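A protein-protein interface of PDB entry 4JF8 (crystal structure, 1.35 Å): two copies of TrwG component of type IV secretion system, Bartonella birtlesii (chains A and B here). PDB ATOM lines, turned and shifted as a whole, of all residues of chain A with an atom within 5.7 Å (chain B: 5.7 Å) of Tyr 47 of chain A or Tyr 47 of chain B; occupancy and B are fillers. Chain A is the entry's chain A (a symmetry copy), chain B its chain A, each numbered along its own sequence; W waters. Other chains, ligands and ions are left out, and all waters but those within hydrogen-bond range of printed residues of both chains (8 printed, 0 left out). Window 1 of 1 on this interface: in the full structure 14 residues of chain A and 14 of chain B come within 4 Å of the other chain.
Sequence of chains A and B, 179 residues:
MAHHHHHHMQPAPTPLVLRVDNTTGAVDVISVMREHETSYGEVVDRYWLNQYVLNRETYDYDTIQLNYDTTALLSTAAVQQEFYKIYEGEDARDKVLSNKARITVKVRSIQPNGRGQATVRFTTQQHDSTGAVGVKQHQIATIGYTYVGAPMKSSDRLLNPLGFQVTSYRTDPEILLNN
The side-chain hydroxyl (OH) of Tyr 47 of chain B is in hydrogen-bond range of the side-chain hydroxyl (OH) of Tyr 47 of chain A (2.6 Å).
Arg 46 of chain A touches Leu 158 of chain B, and with the chains exchanged Leu 158 of chain A touches Arg 46 of chain B.
Tyr 47 of chain A touches its own counterpart, Tyr 47 of chain B.
Tyr 47 of chain A touches Gln 51 of chain B, and with the chains exchanged Gln 51 of chain A touches Tyr 47 of chain B.
Tyr 47 of chain A touches Leu 159 of chain B, and with the chains exchanged Leu 159 of chain A touches Tyr 47 of chain B.
The side-chain hydroxyl of Tyr 47 of chain A sits at hydrogen-bond distance from the side-chain amide nitrogen of Gln 51 of chain A (3.4 Å).
The guanidinium group (NH2) of Arg 46 of chain B lies within salt-bridge range of the side-chain carboxylate (OE1) of Glu 42 of chain B (3.1 Å).
OH of Tyr 47 of chain B sits at hydrogen-bond distance from NE2 of Gln 51 of chain B.
Of the 16 printed residues of chain B, 9 touch a printed residue of chain A.
Hydrophobic or aromatic side chains of chain B within 4 Å of the printed part of chain A: Val 43, Tyr 47, Trp 48, Leu 158 and Pro 161.
Among the printed residues, 17 pairs touch across the chains.
Among the printed residues, no Asp or Glu carboxylate lies within 4 Å of a Lys or Arg side-chain nitrogen of the other chain.
Among the printed residues, merely in contact across the chains: Val 43 of chain A with Arg 157 of chain B, Val 43 of chain A with Pro 161 of chain B, Arg 46 of chain A with Leu 158 of chain B, Tyr 47 of chain A with Trp 48 of chain B, Tyr 47 of chain A with Gln 51 of chain B, Tyr 47 of chain A with Leu 158 of chain B, Tyr 47 of chain A with Leu 159 of chain B, Tyr 47 of chain A with Pro 161 of chain B, Trp 48 of chain A with Tyr 47 of chain B, Gln 51 of chain A with Tyr 47 of chain B, Arg 157 of chain A with Val 43 of chain B, Leu 158 of chain A with Arg 46 of chain B, Leu 158 of chain A with Tyr 47 of chain B, Leu 159 of chain A with Tyr 47 of chain B, Pro 161 of chain A with Val 43 of chain B and Pro 161 of chain A with Tyr 47 of chain B.
Of chain B, only Tyr 47, Trp 48, Gln 51, Leu 158, Leu 159 and Pro 161 come within 4 Å of Tyr 47 of chain A.
Of the printed residues of chain B, Trp 48 of chain A touches Tyr 47.
Printed residues of chain A within 4 Å of Val 43 of chain B: Arg 157 (3.8 Å) and Pro 161 (3.4 Å).
Of the printed residues of chain A, Arg 157 of chain B touches Val 43.
Of the printed residues of chain A, Leu 159 of chain B touches Tyr 47 (3.6 Å).
The nearest printed residue of chain A that does not touch Arg 46 of chain B is Arg 157 of chain A (5.9 Å).
Water W2 lies within hydrogen-bond range of O of Leu 158 of chain B (2.7 Å), O of Tyr 47 of chain A (2.8 Å) and ND2 of Asn 50 of chain A (3.0 Å).
Water W4 lies within hydrogen-bond range of the guanidinium group (NH2) of Arg 157 of chain B (2.9 Å) and the guanidinium group (NH1) of Arg 46 of chain A (3.3 Å).
Water W6 lies within hydrogen-bond range of NH1 of Arg 46 of chain A (3.1 Å) and NE of Arg 157 of chain B (3.2 Å).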
ATOM      1  N   GLU A  42       1.226  -0.853   6.749  1.00  0.00           N
ATOM      2  CA  GLU A  42       1.357  -0.488   5.356  1.00  0.00           C
ATOM      3  C   GLU A  42       0.029  -0.534   4.612  1.00  0.00           C
ATOM      4  O   GLU A  42      -0.276   0.360   3.830  1.00  0.00           O
ATOM      5  CB  GLU A  42       2.396  -1.355   4.622  1.00  0.00           C
ATOM      6  CG  GLU A  42       2.765  -0.776   3.263  1.00  0.00           C
ATOM      7  CD  GLU A  42       3.957  -1.425   2.594  1.00  0.00           C
ATOM      8  OE1 GLU A  42       4.844  -0.669   2.129  1.00  0.00           O
ATOM      9  OE2 GLU A  42       3.972  -2.668   2.493  1.00  0.00           O
ATOM     10  N   VAL A  43      -0.746  -1.589   4.817  1.00  0.00           N
ATOM     11  CA  VAL A  43      -1.977  -1.784   4.041  1.00  0.00           C
ATOM     12  C   VAL A  43      -3.033  -0.719   4.389  1.00  0.00           C
ATOM     13  O   VAL A  43      -3.672  -0.142   3.503  1.00  0.00           O
ATOM     14  CB  VAL A  43      -2.501  -3.243   4.186  1.00  0.00           C
ATOM     15  CG1 VAL A  43      -3.831  -3.412   3.507  1.00  0.00           C
ATOM     16  CG2 VAL A  43      -1.515  -4.227   3.578  1.00  0.00           C
ATOM     17  N   VAL A  44      -3.217  -0.438   5.670  1.00  0.00           N
ATOM     18  CA  VAL A  44      -4.176   0.579   6.075  1.00  0.00           C
ATOM     19  C   VAL A  44      -3.692   1.977   5.702  1.00  0.00           C
ATOM     20  O   VAL A  44      -4.471   2.787   5.184  1.00  0.00           O
ATOM     21  CB  VAL A  44      -4.554   0.457   7.561  1.00  0.00           C
ATOM     22  CG1 VAL A  44      -5.345   1.666   8.013  1.00  0.00           C
ATOM     23  CG2 VAL A  44      -5.330  -0.850   7.776  1.00  0.00           C
ATOM     24  N   ASP A  45      -2.413   2.277   5.894  1.00  0.00           N
ATOM     25  CA  ASP A  45      -1.920   3.594   5.535  1.00  0.00           C
ATOM     26  C   ASP A  45      -2.089   3.792   4.016  1.00  0.00           C
ATOM     27  O   ASP A  45      -2.504   4.857   3.555  1.00  0.00           O
ATOM     28  CB  ASP A  45      -0.450   3.777   5.898  1.00  0.00           C
ATOM     29  CG  ASP A  45      -0.196   3.915   7.387  1.00  0.00           C
ATOM     30  OD1 ASP A  45      -1.104   3.809   8.225  1.00  0.00           O
ATOM     31  OD2 ASP A  45       1.015   4.090   7.737  1.00  0.00           O
ATOM     32  N   ARG A  46      -1.780   2.768   3.220  1.00  0.00           N
ATOM     33  CA  ARG A  46      -1.942   2.874   1.764  1.00  0.00           C
ATOM     34  C   ARG A  46      -3.398   3.129   1.382  1.00  0.00           C
ATOM     35  O   ARG A  46      -3.662   3.904   0.476  1.00  0.00           O
ATOM     36  CB  ARG A  46      -1.415   1.633   1.039  1.00  0.00           C
ATOM     37  CG  ARG A  46       0.104   1.575   0.955  1.00  0.00           C
ATOM     38  CD  ARG A  46       0.560   0.358   0.188  1.00  0.00           C
ATOM     39  NE  ARG A  46       1.954   0.514  -0.217  1.00  0.00           N
ATOM     40  CZ  ARG A  46       2.795  -0.475  -0.499  1.00  0.00           C
ATOM     41  NH1 ARG A  46       2.421  -1.749  -0.412  1.00  0.00           N
ATOM     42  NH2 ARG A  46       4.035  -0.174  -0.849  1.00  0.00           N
ATOM     43  N   TYR A  47      -4.341   2.494   2.080  1.00  0.00           N
ATOM     44  CA  TYR A  47      -5.765   2.735   1.817  1.00  0.00           C
ATOM     45  C   TYR A  47      -6.082   4.222   1.965  1.00  0.00           C
ATOM     46  O   TYR A  47      -6.691   4.827   1.060  1.00  0.00           O
ATOM     47  CB  TYR A  47      -6.632   1.911   2.765  1.00  0.00           C
ATOM     48  CG  TYR A  47      -8.102   2.231   2.663  1.00  0.00           C
ATOM     49  CD1 TYR A  47      -8.875   1.684   1.658  1.00  0.00           C
ATOM     50  CD2 TYR A  47      -8.711   3.144   3.534  1.00  0.00           C
ATOM     51  CE1 TYR A  47     -10.225   1.984   1.538  1.00  0.00           C
ATOM     52  CE2 TYR A  47     -10.060   3.457   3.421  1.00  0.00           C
ATOM     53  CZ  TYR A  47     -10.802   2.883   2.409  1.00  0.00           C
ATOM     54  OH  TYR A  47     -12.140   3.185   2.264  1.00  0.00           O
ATOM     55  N   TRP A  48      -5.690   4.817   3.082  1.00  0.00           N
ATOM     56  CA  TRP A  48      -5.995   6.227   3.336  1.00  0.00           C
ATOM     57  C   TRP A  48      -5.244   7.186   2.417  1.00  0.00           C
ATOM     58  O   TRP A  48      -5.823   8.158   1.921  1.00  0.00           O
ATOM     59  CB  TRP A  48      -5.808   6.592   4.818  1.00  0.00           C
ATOM     60  CG  TRP A  48      -6.875   5.942   5.633  1.00  0.00           C
ATOM     61  CD1 TRP A  48      -6.729   4.877   6.479  1.00  0.00           C
ATOM     62  CD2 TRP A  48      -8.268   6.264   5.624  1.00  0.00           C
ATOM     63  NE1 TRP A  48      -7.951   4.520   6.988  1.00  0.00           N
ATOM     64  CE2 TRP A  48      -8.917   5.347   6.474  1.00  0.00           C
ATOM     65  CE3 TRP A  48      -9.038   7.220   4.949  1.00  0.00           C
ATOM     66  CZ2 TRP A  48     -10.308   5.378   6.669  1.00  0.00           C
ATOM     67  CZ3 TRP A  48     -10.396   7.249   5.169  1.00  0.00           C
ATOM     68  CH2 TRP A  48     -11.013   6.338   6.014  1.00  0.00           C
ATOM     69  N   LEU A  49      -3.972   6.897   2.159  1.00  0.00           N
ATOM     70  CA  LEU A  49      -3.186   7.716   1.248  1.00  0.00           C
ATOM     71  C   LEU A  49      -3.751   7.683  -0.159  1.00  0.00           C
ATOM     72  O   LEU A  49      -3.794   8.710  -0.837  1.00  0.00           O
ATOM     73  CB  LEU A  49      -1.730   7.247   1.247  1.00  0.00           C
ATOM     74  CG  LEU A  49      -0.995   7.534   2.572  1.00  0.00           C
ATOM     75  CD1 LEU A  49       0.246   6.648   2.702  1.00  0.00           C
ATOM     76  CD2 LEU A  49      -0.650   9.010   2.756  1.00  0.00           C
ATOM     77  N   ASN A  50      -4.139   6.499  -0.605  1.00  0.00           N
ATOM     78  CA  ASN A  50      -4.765   6.350  -1.910  1.00  0.00           C
ATOM     79  C   ASN A  50      -6.071   7.146  -1.985  1.00  0.00           C
ATOM     80  O   ASN A  50      -6.324   7.877  -2.955  1.00  0.00           O
ATOM     81  CB  ASN A  50      -5.010   4.860  -2.179  1.00  0.00           C
ATOM     82  CG  ASN A  50      -5.545   4.588  -3.555  1.00  0.00           C
ATOM     83  OD1 ASN A  50      -4.880   4.892  -4.549  1.00  0.00           O
ATOM     84  ND2 ASN A  50      -6.718   3.959  -3.637  1.00  0.00           N
ATOM     85  N   GLN A  51      -6.916   6.988  -0.971  1.00  0.00           N
ATOM     86  CA  GLN A  51      -8.177   7.716  -0.957  1.00  0.00           C
ATOM     87  C   GLN A  51      -7.893   9.212  -1.020  1.00  0.00           C
ATOM     88  O   GLN A  51      -8.570   9.962  -1.735  1.00  0.00           O
ATOM     89  CB  GLN A  51      -8.939   7.404   0.322  1.00  0.00           C
ATOM     90  CG  GLN A  51     -10.288   8.096   0.368  1.00  0.00           C
ATOM     91  CD  GLN A  51     -11.160   7.701   1.552  1.00  0.00           C
ATOM     92  OE1 GLN A  51     -11.566   8.541   2.355  1.00  0.00           O
ATOM     93  NE2 GLN A  51     -11.433   6.425   1.672  1.00  0.00           N
ATOM     94  N   TYR A  52      -6.881   9.679  -0.289  1.00  0.00           N
ATOM     95  CA  TYR A  52      -6.571  11.091  -0.271  1.00  0.00           C
ATOM     96  C   TYR A  52      -6.146  11.618  -1.638  1.00  0.00           C
ATOM     97  O   TYR A  52      -6.694  12.613  -2.120  1.00  0.00           O
ATOM     98  CB  TYR A  52      -5.489  11.401   0.777  1.00  0.00           C
ATOM     99  CG  TYR A  52      -5.365  12.888   1.038  1.00  0.00           C
ATOM    100  CD1 TYR A  52      -6.282  13.521   1.876  1.00  0.00           C
ATOM    101  CD2 TYR A  52      -4.402  13.680   0.397  1.00  0.00           C
ATOM    102  CE1 TYR A  52      -6.230  14.885   2.109  1.00  0.00           C
ATOM    103  CE2 TYR A  52      -4.344  15.041   0.630  1.00  0.00           C
ATOM    104  CZ  TYR A  52      -5.270  15.641   1.466  1.00  0.00           C
ATOM    105  OH  TYR A  52      -5.168  17.010   1.707  1.00  0.00           O
ATOM    106  N   ARG A 157     -16.958  10.752  12.209  1.00  0.00           N
ATOM    107  CA  ARG A 157     -16.427   9.478  12.657  1.00  0.00           C
ATOM    108  C   ARG A 157     -16.821   8.341  11.707  1.00  0.00           C
ATOM    109  O   ARG A 157     -16.049   7.405  11.478  1.00  0.00           O
ATOM    110  CB  ARG A 157     -16.950   9.222  14.052  1.00  0.00           C
ATOM    111  CG  ARG A 157     -16.352   8.034  14.744  1.00  0.00           C
ATOM    112  CD  ARG A 157     -16.591   8.122  16.241  1.00  0.00           C
ATOM    113  NE  ARG A 157     -17.993   8.217  16.641  1.00  0.00           N
ATOM    114  CZ  ARG A 157     -18.563   9.265  17.242  1.00  0.00           C
ATOM    115  NH1 ARG A 157     -17.904  10.393  17.459  1.00  0.00           N
ATOM    116  NH2 ARG A 157     -19.842   9.190  17.606  1.00  0.00           N
ATOM    117  N   LEU A 158     -18.001   8.443  11.096  1.00  0.00           N
ATOM    118  CA  LEU A 158     -18.469   7.430  10.151  1.00  0.00           C
ATOM    119  C   LEU A 158     -17.659   7.413   8.868  1.00  0.00           C
ATOM    120  O   LEU A 158     -17.649   6.399   8.167  1.00  0.00           O
ATOM    121  CB  LEU A 158     -19.932   7.656   9.792  1.00  0.00           C
ATOM    122  CG  LEU A 158     -20.984   7.094  10.720  1.00  0.00           C
ATOM    123  CD1 LEU A 158     -22.358   7.487  10.204  1.00  0.00           C
ATOM    124  CD2 LEU A 158     -20.857   5.572  10.797  1.00  0.00           C
ATOM    125  N   LEU A 159     -17.012   8.524   8.521  1.00  0.00           N
ATOM    126  CA  LEU A 159     -16.225   8.612   7.295  1.00  0.00           C
ATOM    127  C   LEU A 159     -14.727   8.678   7.540  1.00  0.00           C
ATOM    128  O   LEU A 159     -13.941   8.588   6.613  1.00  0.00           O
ATOM    129  CB  LEU A 159     -16.671   9.824   6.453  1.00  0.00           C
ATOM    130  CG  LEU A 159     -18.094   9.733   5.909  1.00  0.00           C
ATOM    131  CD1 LEU A 159     -18.540  11.065   5.300  1.00  0.00           C
ATOM    132  CD2 LEU A 159     -18.177   8.601   4.918  1.00  0.00           C
ATOM    133  N   ASN A 160     -14.323   8.854   8.803  1.00  0.00           N
ATOM    134  CA  ASN A 160     -12.895   8.905   9.130  1.00  0.00           C
ATOM    135  C   ASN A 160     -12.649   8.261  10.493  1.00  0.00           C
ATOM    136  O   ASN A 160     -12.304   8.935  11.457  1.00  0.00           O
ATOM    137  CB  ASN A 160     -12.390  10.344   9.101  1.00  0.00           C
ATOM    138  CG  ASN A 160     -10.884  10.441   9.259  1.00  0.00           C
ATOM    139  OD1 ASN A 160     -10.163   9.462   9.116  1.00  0.00           O
ATOM    140  ND2 ASN A 160     -10.406  11.628   9.517  1.00  0.00           N
ATOM    141  N   PRO A 161     -12.839   6.944  10.578  1.00  0.00           N
ATOM    142  CA  PRO A 161     -12.941   6.248  11.875  1.00  0.00           C
ATOM    143  C   PRO A 161     -11.699   6.370  12.752  1.00  0.00           C
ATOM    144  O   PRO A 161     -11.837   6.386  13.968  1.00  0.00           O
ATOM    145  CB  PRO A 161     -13.199   4.786  11.471  1.00  0.00           C
ATOM    146  CG  PRO A 161     -12.722   4.692  10.046  1.00  0.00           C
ATOM    147  CD  PRO A 161     -13.090   6.024   9.465  1.00  0.00           C
ATOM    148  N   GLU B  42     -16.360  -1.259  17.028  1.00  0.00           N
ATOM    149  CA  GLU B  42     -17.575  -0.592  16.609  1.00  0.00           C
ATOM    150  C   GLU B  42     -17.321   0.476  15.554  1.00  0.00           C
ATOM    151  O   GLU B  42     -18.063   0.579  14.583  1.00  0.00           O
ATOM    152  CB  GLU B  42     -18.342   0.017  17.795  1.00  0.00           C
ATOM    153  CG  GLU B  42     -19.755   0.431  17.406  1.00  0.00           C
ATOM    154  CD  GLU B  42     -20.654   0.801  18.567  1.00  0.00           C
ATOM    155  OE1 GLU B  42     -21.801   0.292  18.598  1.00  0.00           O
ATOM    156  OE2 GLU B  42     -20.233   1.628  19.399  1.00  0.00           O
ATOM    157  N   VAL B  43     -16.303   1.300  15.757  1.00  0.00           N
ATOM    158  CA  VAL B  43     -16.068   2.443  14.866  1.00  0.00           C
ATOM    159  C   VAL B  43     -15.643   1.980  13.460  1.00  0.00           C
ATOM    160  O   VAL B  43     -16.141   2.482  12.446  1.00  0.00           O
ATOM    161  CB  VAL B  43     -15.074   3.454  15.508  1.00  0.00           C
ATOM    162  CG1 VAL B  43     -14.723   4.556  14.547  1.00  0.00           C
ATOM    163  CG2 VAL B  43     -15.675   4.071  16.759  1.00  0.00           C
ATOM    164  N   VAL B  44     -14.741   1.014  13.382  1.00  0.00           N
ATOM    165  CA  VAL B  44     -14.312   0.502  12.089  1.00  0.00           C
ATOM    166  C   VAL B  44     -15.422  -0.301  11.416  1.00  0.00           C
ATOM    167  O   VAL B  44     -15.669  -0.133  10.215  1.00  0.00           O
ATOM    168  CB  VAL B  44     -12.989  -0.276  12.185  1.00  0.00           C
ATOM    169  CG1 VAL B  44     -12.702  -1.006  10.890  1.00  0.00           C
ATOM    170  CG2 VAL B  44     -11.862   0.696  12.559  1.00  0.00           C
ATOM    171  N   ASP B  45     -16.141  -1.132  12.159  1.00  0.00           N
ATOM    172  CA  ASP B  45     -17.215  -1.899  11.550  1.00  0.00           C
ATOM    173  C   ASP B  45     -18.277  -0.924  11.008  1.00  0.00           C
ATOM    174  O   ASP B  45     -18.797  -1.099   9.904  1.00  0.00           O
ATOM    175  CB  ASP B  45     -17.875  -2.852  12.540  1.00  0.00           C
ATOM    176  CG  ASP B  45     -17.018  -4.048  12.911  1.00  0.00           C
ATOM    177  OD1 ASP B  45     -15.857  -4.182  12.495  1.00  0.00           O
ATOM    178  OD2 ASP B  45     -17.537  -4.881  13.719  1.00  0.00           O
ATOM    179  N   ARG B  46     -18.606   0.119  11.769  1.00  0.00           N
ATOM    180  CA  ARG B  46     -19.591   1.105  11.305  1.00  0.00           C
ATOM    181  C   ARG B  46     -19.129   1.795  10.024  1.00  0.00           C
ATOM    182  O   ARG B  46     -19.935   2.039   9.139  1.00  0.00           O
ATOM    183  CB  ARG B  46     -19.908   2.146  12.382  1.00  0.00           C
ATOM    184  CG  ARG B  46     -20.818   1.624  13.485  1.00  0.00           C
ATOM    185  CD  ARG B  46     -21.133   2.707  14.488  1.00  0.00           C
ATOM    186  NE  ARG B  46     -22.286   2.322  15.296  1.00  0.00           N
ATOM    187  CZ  ARG B  46     -22.570   2.780  16.510  1.00  0.00           C
ATOM    188  NH1 ARG B  46     -21.779   3.657  17.123  1.00  0.00           N
ATOM    189  NH2 ARG B  46     -23.655   2.331  17.121  1.00  0.00           N
ATOM    190  N   TYR B  47     -17.833   2.096   9.916  1.00  0.00           N
ATOM    191  CA  TYR B  47     -17.299   2.701   8.690  1.00  0.00           C
ATOM    192  C   TYR B  47     -17.613   1.815   7.487  1.00  0.00           C
ATOM    193  O   TYR B  47     -18.151   2.302   6.471  1.00  0.00           O
ATOM    194  CB  TYR B  47     -15.793   2.917   8.812  1.00  0.00           C
ATOM    195  CG  TYR B  47     -15.150   3.383   7.531  1.00  0.00           C
ATOM    196  CD1 TYR B  47     -15.199   4.713   7.160  1.00  0.00           C
ATOM    197  CD2 TYR B  47     -14.549   2.479   6.645  1.00  0.00           C
ATOM    198  CE1 TYR B  47     -14.629   5.156   5.974  1.00  0.00           C
ATOM    199  CE2 TYR B  47     -13.981   2.908   5.452  1.00  0.00           C
ATOM    200  CZ  TYR B  47     -14.042   4.247   5.121  1.00  0.00           C
ATOM    201  OH  TYR B  47     -13.497   4.700   3.937  1.00  0.00           O
ATOM    202  N   TRP B  48     -17.284   0.534   7.574  1.00  0.00           N
ATOM    203  CA  TRP B  48     -17.500  -0.382   6.452  1.00  0.00           C
ATOM    204  C   TRP B  48     -18.973  -0.653   6.162  1.00  0.00           C
ATOM    205  O   TRP B  48     -19.386  -0.681   4.998  1.00  0.00           O
ATOM    206  CB  TRP B  48     -16.701  -1.684   6.619  1.00  0.00           C
ATOM    207  CG  TRP B  48     -15.245  -1.405   6.455  1.00  0.00           C
ATOM    208  CD1 TRP B  48     -14.296  -1.381   7.440  1.00  0.00           C
ATOM    209  CD2 TRP B  48     -14.580  -1.033   5.244  1.00  0.00           C
ATOM    210  NE1 TRP B  48     -13.087  -1.013   6.910  1.00  0.00           N
ATOM    211  CE2 TRP B  48     -13.232  -0.782   5.566  1.00  0.00           C
ATOM    212  CE3 TRP B  48     -15.004  -0.853   3.922  1.00  0.00           C
ATOM    213  CZ2 TRP B  48     -12.305  -0.371   4.592  1.00  0.00           C
ATOM    214  CZ3 TRP B  48     -14.078  -0.471   2.979  1.00  0.00           C
ATOM    215  CH2 TRP B  48     -12.755  -0.232   3.317  1.00  0.00           C
ATOM    216  N   LEU B  49     -19.771  -0.815   7.213  1.00  0.00           N
ATOM    217  CA  LEU B  49     -21.202  -1.020   7.045  1.00  0.00           C
ATOM    218  C   LEU B  49     -21.864   0.181   6.397  1.00  0.00           C
ATOM    219  O   LEU B  49     -22.737   0.026   5.543  1.00  0.00           O
ATOM    220  CB  LEU B  49     -21.850  -1.320   8.397  1.00  0.00           C
ATOM    221  CG  LEU B  49     -21.447  -2.690   8.978  1.00  0.00           C
ATOM    222  CD1 LEU B  49     -21.709  -2.736  10.484  1.00  0.00           C
ATOM    223  CD2 LEU B  49     -22.111  -3.862   8.258  1.00  0.00           C
ATOM    224  N   ASN B  50     -21.479   1.368   6.838  1.00  0.00           N
ATOM    225  CA  ASN B  50     -21.987   2.596   6.246  1.00  0.00           C
ATOM    226  C   ASN B  50     -21.611   2.686   4.764  1.00  0.00           C
ATOM    227  O   ASN B  50     -22.452   2.995   3.905  1.00  0.00           O
ATOM    228  CB  ASN B  50     -21.435   3.794   7.029  1.00  0.00           C
ATOM    229  CG  ASN B  50     -21.996   5.109   6.572  1.00  0.00           C
ATOM    230  OD1 ASN B  50     -23.208   5.326   6.650  1.00  0.00           O
ATOM    231  ND2 ASN B  50     -21.124   6.026   6.147  1.00  0.00           N
ATOM    232  N   GLN B  51     -20.340   2.438   4.463  1.00  0.00           N
ATOM    233  CA  GLN B  51     -19.900   2.491   3.076  1.00  0.00           C
ATOM    234  C   GLN B  51     -20.713   1.500   2.254  1.00  0.00           C
ATOM    235  O   GLN B  51     -21.136   1.796   1.128  1.00  0.00           O
ATOM    236  CB  GLN B  51     -18.425   2.126   2.989  1.00  0.00           C
ATOM    237  CG  GLN B  51     -17.896   2.214   1.569  1.00  0.00           C
ATOM    238  CD  GLN B  51     -16.393   2.008   1.442  1.00  0.00           C
ATOM    239  OE1 GLN B  51     -15.930   1.113   0.737  1.00  0.00           O
ATOM    240  NE2 GLN B  51     -15.635   2.823   2.134  1.00  0.00           N
ATOM    241  N   TYR B  52     -20.963   0.308   2.796  1.00  0.00           N
ATOM    242  CA  TYR B  52     -21.701  -0.698   2.064  1.00  0.00           C
ATOM    243  C   TYR B  52     -23.130  -0.268   1.750  1.00  0.00           C
ATOM    244  O   TYR B  52     -23.560  -0.332   0.595  1.00  0.00           O
ATOM    245  CB  TYR B  52     -21.703  -2.035   2.823  1.00  0.00           C
ATOM    246  CG  TYR B  52     -22.190  -3.178   1.954  1.00  0.00           C
ATOM    247  CD1 TYR B  52     -21.323  -3.762   1.033  1.00  0.00           C
ATOM    248  CD2 TYR B  52     -23.519  -3.620   1.981  1.00  0.00           C
ATOM    249  CE1 TYR B  52     -21.738  -4.780   0.190  1.00  0.00           C
ATOM    250  CE2 TYR B  52     -23.938  -4.637   1.145  1.00  0.00           C
ATOM    251  CZ  TYR B  52     -23.054  -5.198   0.240  1.00  0.00           C
ATOM    252  OH  TYR B  52     -23.495  -6.244  -0.569  1.00  0.00           O
ATOM    253  N   ARG B 157      -6.715  -4.736  -2.721  1.00  0.00           N
ATOM    254  CA  ARG B 157      -6.187  -4.470  -1.396  1.00  0.00           C
ATOM    255  C   ARG B 157      -6.176  -2.969  -1.087  1.00  0.00           C
ATOM    256  O   ARG B 157      -6.405  -2.550   0.052  1.00  0.00           O
ATOM    257  CB  ARG B 157      -4.790  -5.045  -1.330  1.00  0.00           C
ATOM    258  CG  ARG B 157      -4.162  -5.026   0.032  1.00  0.00           C
ATOM    259  CD  ARG B 157      -2.995  -5.996   0.086  1.00  0.00           C
ATOM    260  NE  ARG B 157      -1.943  -5.758  -0.898  1.00  0.00           N
ATOM    261  CZ  ARG B 157      -1.612  -6.580  -1.899  1.00  0.00           C
ATOM    262  NH1 ARG B 157      -2.293  -7.686  -2.154  1.00  0.00           N
ATOM    263  NH2 ARG B 157      -0.587  -6.262  -2.688  1.00  0.00           N
ATOM    264  N   LEU B 158      -5.973  -2.140  -2.112  1.00  0.00           N
ATOM    265  CA  LEU B 158      -5.966  -0.688  -1.938  1.00  0.00           C
ATOM    266  C   LEU B 158      -7.338  -0.137  -1.595  1.00  0.00           C
ATOM    267  O   LEU B 158      -7.431   0.957  -1.035  1.00  0.00           O
ATOM    268  CB  LEU B 158      -5.471   0.007  -3.200  1.00  0.00           C
ATOM    269  CG  LEU B 158      -3.979   0.150  -3.391  1.00  0.00           C
ATOM    270  CD1 LEU B 158      -3.715   0.814  -4.732  1.00  0.00           C
ATOM    271  CD2 LEU B 158      -3.382   0.983  -2.257  1.00  0.00           C
ATOM    272  N   LEU B 159      -8.406  -0.847  -1.953  1.00  0.00           N
ATOM    273  CA  LEU B 159      -9.766  -0.391  -1.685  1.00  0.00           C
ATOM    274  C   LEU B 159     -10.479  -1.202  -0.618  1.00  0.00           C
ATOM    275  O   LEU B 159     -11.555  -0.837  -0.175  1.00  0.00           O
ATOM    276  CB  LEU B 159     -10.598  -0.385  -2.982  1.00  0.00           C
ATOM    277  CG  LEU B 159     -10.129   0.615  -4.037  1.00  0.00           C
ATOM    278  CD1 LEU B 159     -10.845   0.388  -5.371  1.00  0.00           C
ATOM    279  CD2 LEU B 159     -10.329   2.016  -3.518  1.00  0.00           C
ATOM    280  N   ASN B 160      -9.885  -2.329  -0.209  1.00  0.00           N
ATOM    281  CA  ASN B 160     -10.495  -3.159   0.833  1.00  0.00           C
ATOM    282  C   ASN B 160      -9.406  -3.785   1.703  1.00  0.00           C
ATOM    283  O   ASN B 160      -9.192  -4.992   1.676  1.00  0.00           O
ATOM    284  CB  ASN B 160     -11.388  -4.229   0.212  1.00  0.00           C
ATOM    285  CG  ASN B 160     -12.181  -5.005   1.248  1.00  0.00           C
ATOM    286  OD1 ASN B 160     -12.301  -4.597   2.396  1.00  0.00           O
ATOM    287  ND2 ASN B 160     -12.751  -6.103   0.834  1.00  0.00           N
ATOM    288  N   PRO B 161      -8.703  -2.956   2.476  1.00  0.00           N
ATOM    289  CA  PRO B 161      -7.441  -3.365   3.120  1.00  0.00           C
ATOM    290  C   PRO B 161      -7.581  -4.536   4.088  1.00  0.00           C
ATOM    291  O   PRO B 161      -6.644  -5.313   4.210  1.00  0.00           O
ATOM    292  CB  PRO B 161      -6.989  -2.088   3.850  1.00  0.00           C
ATOM    293  CG  PRO B 161      -8.239  -1.258   3.982  1.00  0.00           C
ATOM    294  CD  PRO B 161      -8.978  -1.536   2.708  1.00  0.00           C
HETATM  295  O   HOH W   1     -17.322   4.928  12.119  1.00  0.00           O
HETATM  296  O   HOH W   2      -8.101   3.570  -0.978  1.00  0.00           O
HETATM  297  O   HOH W   3     -19.213   5.255  16.673  1.00  0.00           O
HETATM  298  O   HOH W   4       0.859  -3.799  -2.491  1.00  0.00           O
HETATM  299  O   HOH W   5      -4.214  -0.947   0.945  1.00  0.00           O
HETATM  300  O   HOH W   6      -0.020  -3.465   0.244  1.00  0.00           O
HETATM  301  O   HOH W   7     -21.529   6.956  17.005  1.00  0.00           O
HETATM  302  O   HOH W   8     -18.280   5.025   5.933  1.00  0.00           O
